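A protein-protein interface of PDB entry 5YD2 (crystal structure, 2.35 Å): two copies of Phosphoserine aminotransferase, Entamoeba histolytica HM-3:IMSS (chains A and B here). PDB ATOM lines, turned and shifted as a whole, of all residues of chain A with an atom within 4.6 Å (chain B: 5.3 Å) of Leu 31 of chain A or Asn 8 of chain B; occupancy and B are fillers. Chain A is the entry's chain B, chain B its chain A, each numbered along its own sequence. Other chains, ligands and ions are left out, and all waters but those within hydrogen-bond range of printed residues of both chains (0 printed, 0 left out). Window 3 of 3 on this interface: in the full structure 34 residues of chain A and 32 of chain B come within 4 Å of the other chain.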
ATOM      1  N   ASN A  26       5.420  -9.484 -21.786  1.00  0.00           N
ATOM      2  CA  ASN A  26       5.291  -8.232 -21.068  1.00  0.00           C
ATOM      3  C   ASN A  26       3.946  -7.596 -21.312  1.00  0.00           C
ATOM      4  O   ASN A  26       3.738  -6.897 -22.297  1.00  0.00           O
ATOM      5  CB  ASN A  26       6.402  -7.252 -21.472  1.00  0.00           C
ATOM      6  CG  ASN A  26       6.290  -5.889 -20.771  1.00  0.00           C
ATOM      7  OD1 ASN A  26       5.636  -5.740 -19.728  1.00  0.00           O
ATOM      8  ND2 ASN A  26       6.937  -4.888 -21.354  1.00  0.00           N
ATOM      9  N   PHE A  27       3.053  -7.781 -20.359  1.00  0.00           N
ATOM     10  CA  PHE A  27       1.748  -7.157 -20.426  1.00  0.00           C
ATOM     11  C   PHE A  27       1.753  -5.706 -19.933  1.00  0.00           C
ATOM     12  O   PHE A  27       1.144  -4.848 -20.561  1.00  0.00           O
ATOM     13  CB  PHE A  27       0.748  -7.955 -19.594  1.00  0.00           C
ATOM     14  CG  PHE A  27      -0.597  -7.334 -19.558  1.00  0.00           C
ATOM     15  CD1 PHE A  27      -1.293  -7.126 -20.740  1.00  0.00           C
ATOM     16  CD2 PHE A  27      -1.142  -6.887 -18.359  1.00  0.00           C
ATOM     17  CE1 PHE A  27      -2.533  -6.509 -20.730  1.00  0.00           C
ATOM     18  CE2 PHE A  27      -2.376  -6.261 -18.327  1.00  0.00           C
ATOM     19  CZ  PHE A  27      -3.073  -6.077 -19.520  1.00  0.00           C
ATOM     20  N   TRP A  28       2.413  -5.459 -18.796  1.00  0.00           N
ATOM     21  CA  TRP A  28       2.422  -4.140 -18.148  1.00  0.00           C
ATOM     22  C   TRP A  28       3.624  -3.979 -17.227  1.00  0.00           C
ATOM     23  O   TRP A  28       3.786  -4.730 -16.258  1.00  0.00           O
ATOM     24  CB  TRP A  28       1.152  -3.932 -17.318  1.00  0.00           C
ATOM     25  CG  TRP A  28       1.127  -2.634 -16.521  1.00  0.00           C
ATOM     26  CD1 TRP A  28       0.770  -1.384 -16.978  1.00  0.00           C
ATOM     27  CD2 TRP A  28       1.449  -2.471 -15.132  1.00  0.00           C
ATOM     28  NE1 TRP A  28       0.853  -0.467 -15.960  1.00  0.00           N
ATOM     29  CE2 TRP A  28       1.270  -1.103 -14.818  1.00  0.00           C
ATOM     30  CE3 TRP A  28       1.866  -3.353 -14.118  1.00  0.00           C
ATOM     31  CZ2 TRP A  28       1.513  -0.586 -13.526  1.00  0.00           C
ATOM     32  CZ3 TRP A  28       2.101  -2.839 -12.826  1.00  0.00           C
ATOM     33  CH2 TRP A  28       1.924  -1.466 -12.550  1.00  0.00           C
ATOM     34  N   GLU A  29       4.457  -2.990 -17.537  1.00  0.00           N
ATOM     35  CA  GLU A  29       5.556  -2.600 -16.660  1.00  0.00           C
ATOM     36  C   GLU A  29       6.452  -3.801 -16.319  1.00  0.00           C
ATOM     37  O   GLU A  29       6.853  -3.988 -15.180  1.00  0.00           O
ATOM     38  CB  GLU A  29       5.011  -1.898 -15.382  1.00  0.00           C
ATOM     39  CG  GLU A  29       5.875  -0.712 -14.958  1.00  0.00           C
ATOM     40  CD  GLU A  29       5.963  -0.515 -13.450  1.00  0.00           C
ATOM     41  OE1 GLU A  29       7.012  -0.864 -12.856  1.00  0.00           O
ATOM     42  OE2 GLU A  29       4.991   0.000 -12.859  1.00  0.00           O
ATOM     43  N   GLY A  30       6.766  -4.615 -17.323  1.00  0.00           N
ATOM     44  CA  GLY A  30       7.664  -5.767 -17.152  1.00  0.00           C
ATOM     45  C   GLY A  30       7.003  -7.061 -16.707  1.00  0.00           C
ATOM     46  O   GLY A  30       7.596  -8.132 -16.820  1.00  0.00           O
ATOM     47  N   LEU A  31       5.778  -6.962 -16.192  1.00  0.00           N
ATOM     48  CA  LEU A  31       5.032  -8.128 -15.670  1.00  0.00           C
ATOM     49  C   LEU A  31       4.248  -8.878 -16.759  1.00  0.00           C
ATOM     50  O   LEU A  31       3.532  -8.275 -17.571  1.00  0.00           O
ATOM     51  CB  LEU A  31       4.064  -7.689 -14.554  1.00  0.00           C
ATOM     52  CG  LEU A  31       4.619  -7.312 -13.178  1.00  0.00           C
ATOM     53  CD1 LEU A  31       3.464  -7.154 -12.193  1.00  0.00           C
ATOM     54  CD2 LEU A  31       5.600  -8.347 -12.637  1.00  0.00           C
ATOM     55  N   SER A  32       4.393 -10.199 -16.758  1.00  0.00           N
ATOM     56  CA  SER A  32       3.674 -11.065 -17.681  1.00  0.00           C
ATOM     57  C   SER A  32       2.187 -11.030 -17.387  1.00  0.00           C
ATOM     58  O   SER A  32       1.778 -10.912 -16.223  1.00  0.00           O
ATOM     59  CB  SER A  32       4.156 -12.491 -17.530  1.00  0.00           C
ATOM     60  OG  SER A  32       3.199 -13.406 -18.062  1.00  0.00           O
ATOM     61  N   ILE A  33       1.360 -11.158 -18.422  1.00  0.00           N
ATOM     62  CA  ILE A  33      -0.062 -11.315 -18.171  1.00  0.00           C
ATOM     63  C   ILE A  33      -0.364 -12.530 -17.298  1.00  0.00           C
ATOM     64  O   ILE A  33      -1.377 -12.544 -16.601  1.00  0.00           O
ATOM     65  CB  ILE A  33      -0.900 -11.350 -19.443  1.00  0.00           C
ATOM     66  CG1 ILE A  33      -2.384 -11.306 -19.063  1.00  0.00           C
ATOM     67  CG2 ILE A  33      -0.595 -12.577 -20.278  1.00  0.00           C
ATOM     68  CD1 ILE A  33      -3.269 -10.705 -20.125  1.00  0.00           C
ATOM     69  N   GLU A  35       1.193 -13.166 -14.559  1.00  0.00           N
ATOM     70  CA  GLU A  35       1.607 -12.920 -13.168  1.00  0.00           C
ATOM     71  C   GLU A  35       0.980 -11.694 -12.508  1.00  0.00           C
ATOM     72  O   GLU A  35       1.087 -11.532 -11.320  1.00  0.00           O
ATOM     73  CB  GLU A  35       3.131 -12.909 -13.039  1.00  0.00           C
ATOM     74  CG  GLU A  35       3.844 -11.763 -13.721  1.00  0.00           C
ATOM     75  CD  GLU A  35       5.348 -12.007 -13.828  1.00  0.00           C
ATOM     76  OE1 GLU A  35       5.918 -12.782 -13.017  1.00  0.00           O
ATOM     77  OE2 GLU A  35       5.971 -11.432 -14.735  1.00  0.00           O
ATOM     78  N   ILE A  36       0.262 -10.886 -13.273  1.00  0.00           N
ATOM     79  CA  ILE A  36      -0.504  -9.792 -12.698  1.00  0.00           C
ATOM     80  C   ILE A  36      -1.706 -10.307 -11.923  1.00  0.00           C
ATOM     81  O   ILE A  36      -2.185 -11.397 -12.123  1.00  0.00           O
ATOM     82  CB  ILE A  36      -1.008  -8.778 -13.753  1.00  0.00           C
ATOM     83  CG1 ILE A  36      -1.847  -9.476 -14.830  1.00  0.00           C
ATOM     84  CG2 ILE A  36       0.155  -8.005 -14.358  1.00  0.00           C
ATOM     85  CD1 ILE A  36      -3.331  -9.302 -14.625  1.00  0.00           C
ATOM     86  N   ILE B   6      13.628  -4.262 -10.124  1.00  0.00           N
ATOM     87  CA  ILE B   6      12.320  -4.278  -9.380  1.00  0.00           C
ATOM     88  C   ILE B   6      12.082  -5.655  -8.727  1.00  0.00           C
ATOM     89  O   ILE B   6      12.589  -6.682  -9.194  1.00  0.00           O
ATOM     90  CB  ILE B   6      11.121  -3.778 -10.264  1.00  0.00           C
ATOM     91  CG1 ILE B   6      10.956  -2.257 -10.111  1.00  0.00           C
ATOM     92  CG2 ILE B   6       9.792  -4.450  -9.918  1.00  0.00           C
ATOM     93  CD1 ILE B   6       9.940  -1.646 -11.054  1.00  0.00           C
ATOM     94  N   HIS B   7      11.338  -5.628  -7.619  1.00  0.00           N
ATOM     95  CA  HIS B   7      11.107  -6.782  -6.760  1.00  0.00           C
ATOM     96  C   HIS B   7       9.621  -7.107  -6.707  1.00  0.00           C
ATOM     97  O   HIS B   7       8.765  -6.246  -6.447  1.00  0.00           O
ATOM     98  CB  HIS B   7      11.642  -6.514  -5.355  1.00  0.00           C
ATOM     99  CG  HIS B   7      13.015  -5.914  -5.336  1.00  0.00           C
ATOM    100  ND1 HIS B   7      13.229  -4.563  -5.163  1.00  0.00           N
ATOM    101  CD2 HIS B   7      14.243  -6.472  -5.486  1.00  0.00           C
ATOM    102  CE1 HIS B   7      14.526  -4.313  -5.206  1.00  0.00           C
ATOM    103  NE2 HIS B   7      15.164  -5.455  -5.402  1.00  0.00           N
ATOM    104  N   ASN B   8       9.344  -8.386  -6.908  1.00  0.00           N
ATOM    105  CA  ASN B   8       8.076  -8.827  -7.450  1.00  0.00           C
ATOM    106  C   ASN B   8       7.400  -9.886  -6.563  1.00  0.00           C
ATOM    107  O   ASN B   8       7.869 -11.020  -6.477  1.00  0.00           O
ATOM    108  CB  ASN B   8       8.368  -9.369  -8.860  1.00  0.00           C
ATOM    109  CG  ASN B   8       7.119  -9.585  -9.695  1.00  0.00           C
ATOM    110  OD1 ASN B   8       6.007  -9.169  -9.336  1.00  0.00           O
ATOM    111  ND2 ASN B   8       7.302 -10.245 -10.839  1.00  0.00           N
ATOM    112  N   PHE B   9       6.321  -9.482  -5.885  1.00  0.00           N
ATOM    113  CA  PHE B   9       5.474 -10.386  -5.078  1.00  0.00           C
ATOM    114  C   PHE B   9       4.219 -10.802  -5.859  1.00  0.00           C
ATOM    115  O   PHE B   9       3.153 -10.192  -5.739  1.00  0.00           O
ATOM    116  CB  PHE B   9       5.119  -9.712  -3.737  1.00  0.00           C
ATOM    117  CG  PHE B   9       6.266  -9.693  -2.769  1.00  0.00           C
ATOM    118  CD1 PHE B   9       6.432 -10.706  -1.845  1.00  0.00           C
ATOM    119  CD2 PHE B   9       7.217  -8.678  -2.828  1.00  0.00           C
ATOM    120  CE1 PHE B   9       7.503 -10.698  -0.974  1.00  0.00           C
ATOM    121  CE2 PHE B   9       8.291  -8.675  -1.969  1.00  0.00           C
ATOM    122  CZ  PHE B   9       8.437  -9.685  -1.044  1.00  0.00           C
ATOM    123  N   GLY B  10       4.369 -11.878  -6.624  1.00  0.00           N
ATOM    124  CA  GLY B  10       3.530 -12.170  -7.785  1.00  0.00           C
ATOM    125  C   GLY B  10       4.272 -12.991  -8.851  1.00  0.00           C
ATOM    126  O   GLY B  10       3.647 -13.704  -9.650  1.00  0.00           O
ATOM    127  N   ALA B  11       5.606 -12.902  -8.859  1.00  0.00           N
ATOM    128  CA  ALA B  11       6.430 -13.396  -9.962  1.00  0.00           C
ATOM    129  C   ALA B  11       6.115 -14.852 -10.317  1.00  0.00           C
ATOM    130  O   ALA B  11       5.811 -15.667  -9.439  1.00  0.00           O
ATOM    131  CB  ALA B  11       7.921 -13.238  -9.632  1.00  0.00           C
ATOM    132  N   MET B  12       6.154 -15.158 -11.608  1.00  0.00           N
ATOM    133  CA  MET B  12       6.204 -16.550 -12.065  1.00  0.00           C
ATOM    134  C   MET B  12       7.644 -16.776 -12.477  1.00  0.00           C
ATOM    135  O   MET B  12       8.303 -15.838 -12.937  1.00  0.00           O
ATOM    136  CB  MET B  12       5.314 -16.782 -13.291  1.00  0.00           C
ATOM    137  CG  MET B  12       3.822 -16.942 -13.064  1.00  0.00           C
ATOM    138  SD  MET B  12       3.123 -17.908 -14.448  1.00  0.00           S
ATOM    139  CE  MET B  12       3.138 -19.530 -13.660  1.00  0.00           C
ATOM    140  N   ILE B 314       5.412  -4.002  -4.604  1.00  0.00           N
ATOM    141  CA  ILE B 314       4.023  -3.937  -5.072  1.00  0.00           C
ATOM    142  C   ILE B 314       3.184  -5.128  -4.564  1.00  0.00           C
ATOM    143  O   ILE B 314       3.698  -6.254  -4.392  1.00  0.00           O
ATOM    144  CB  ILE B 314       3.928  -3.820  -6.626  1.00  0.00           C
ATOM    145  CG1 ILE B 314       4.415  -5.097  -7.362  1.00  0.00           C
ATOM    146  CG2 ILE B 314       4.648  -2.565  -7.116  1.00  0.00           C
ATOM    147  CD1 ILE B 314       5.913  -5.338  -7.384  1.00  0.00           C
ATOM    148  N   VAL B 333       8.748 -16.108  -6.035  1.00  0.00           N
ATOM    149  CA  VAL B 333       9.242 -14.856  -5.432  1.00  0.00           C
ATOM    150  C   VAL B 333      10.626 -15.096  -4.870  1.00  0.00           C
ATOM    151  O   VAL B 333      10.847 -16.009  -4.086  1.00  0.00           O
ATOM    152  CB  VAL B 333       8.308 -14.322  -4.336  1.00  0.00           C
ATOM    153  CG1 VAL B 333       8.962 -13.149  -3.584  1.00  0.00           C
ATOM    154  CG2 VAL B 333       6.976 -13.932  -4.968  1.00  0.00           C
ATOM    155  N   THR B 334      11.557 -14.269  -5.295  1.00  0.00           N
ATOM    156  CA  THR B 334      12.941 -14.507  -4.978  1.00  0.00           C
ATOM    157  C   THR B 334      13.353 -14.015  -3.588  1.00  0.00           C
ATOM    158  O   THR B 334      12.765 -13.086  -3.014  1.00  0.00           O
ATOM    159  CB  THR B 334      13.878 -13.915  -6.036  1.00  0.00           C
ATOM    160  OG1 THR B 334      15.173 -13.802  -5.445  1.00  0.00           O
ATOM    161  CG2 THR B 334      13.414 -12.526  -6.542  1.00  0.00           C
ATOM    162  N   SER B 337      13.885 -10.277  -3.580  1.00  0.00           N
ATOM    163  CA  SER B 337      12.679  -9.481  -3.421  1.00  0.00           C
ATOM    164  C   SER B 337      12.247  -9.428  -1.964  1.00  0.00           C
ATOM    165  O   SER B 337      11.701  -8.430  -1.518  1.00  0.00           O
ATOM    166  CB  SER B 337      11.555 -10.016  -4.283  1.00  0.00           C
ATOM    167  OG  SER B 337      11.911  -9.878  -5.640  1.00  0.00           O
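The side-chain carboxylate of Glu 35 of chain A sits at hydrogen-bond distance from the backbone NH of Met 12 of chain B (2.8 Å).
OG of Ser 337 of chain B is in hydrogen-bond range of N of Asn 8 of chain B (3.2 Å). The backbone NH (N) of Ser 32 of chain A is in hydrogen-bond range of the side-chain carboxylate (OE2) of Glu 35 of chain A, 2.8 Å away.
Among the printed residues, merely in contact across the chains: Glu 29 of chain A with Ile 6 of chain B (3.5 Å), Leu 31 of chain A with Asn 8 of chain B (3.1 Å), Glu 35 of chain A with Asn 8 of chain B (3.6 Å), Glu 35 of chain A with Gly 10 of chain B (3.5 Å) and Glu 35 of chain A with Ala 11 of chain B (3.2 Å).
Printed residues of chain B within 4 Å of Glu 29 of chain A: Ile 6 (3.5 Å). Leu 31 of chain A touches one residue of chain B. Of the printed residues of chain B, Glu 35 of chain A touches Asn 8, Gly 10, Ala 11 and Met 12. Of the printed residues of chain A, Ile 6 of chain B touches Glu 29. His 7 of chain B touches none of the printed residues of chain A. Of chain A, only Leu 31 and Glu 35 come within 4 Å of Asn 8 of chain B. Printed residues of chain A within 4 Å of Met 12 of chain B: Glu 35. The nearest printed residue of chain B that does not touch Leu 31 of chain A is Ile 314 of chain B (5.3 Å). The nearest printed residue of chain A that does not touch Asn 8 of chain B is Gly 30 of chain A (6.4 Å). The nearest printed residue of chain A that does not touch Gly 10 of chain B is Ile 36 of chain A (5.7 Å).
Of the 11 printed residues of chain B, 5 touch a printed residue of chain A. Printed residues of chain B that touch a printed residue of chain A: Ile 6, Asn 8, Gly 10, Ala 11 and Met 12. Hydrophobic or aromatic side chains of chain B that line the printed part of chain A: Ile 6 and Ala 11. Of the 10 printed residues of chain A, 3 touch a printed residue of chain B. Printed residues of chain A that touch a printed residue of chain B: Glu 29, Leu 31 and Glu 35. Hydrophobic or aromatic side chains of chain A that line the printed part of chain B: Leu 31. Among the printed residues, 6 pairs touch across the chains. Among the printed residues, no Asp or Glu carboxylate lies within 4 Å of a Lys or Arg side-chain nitrogen of the other chain.
No position is printed for both chains. Of the 6 pairs that touch across the chains among the printed residues, none has its exchanged pair printed and touching as well.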
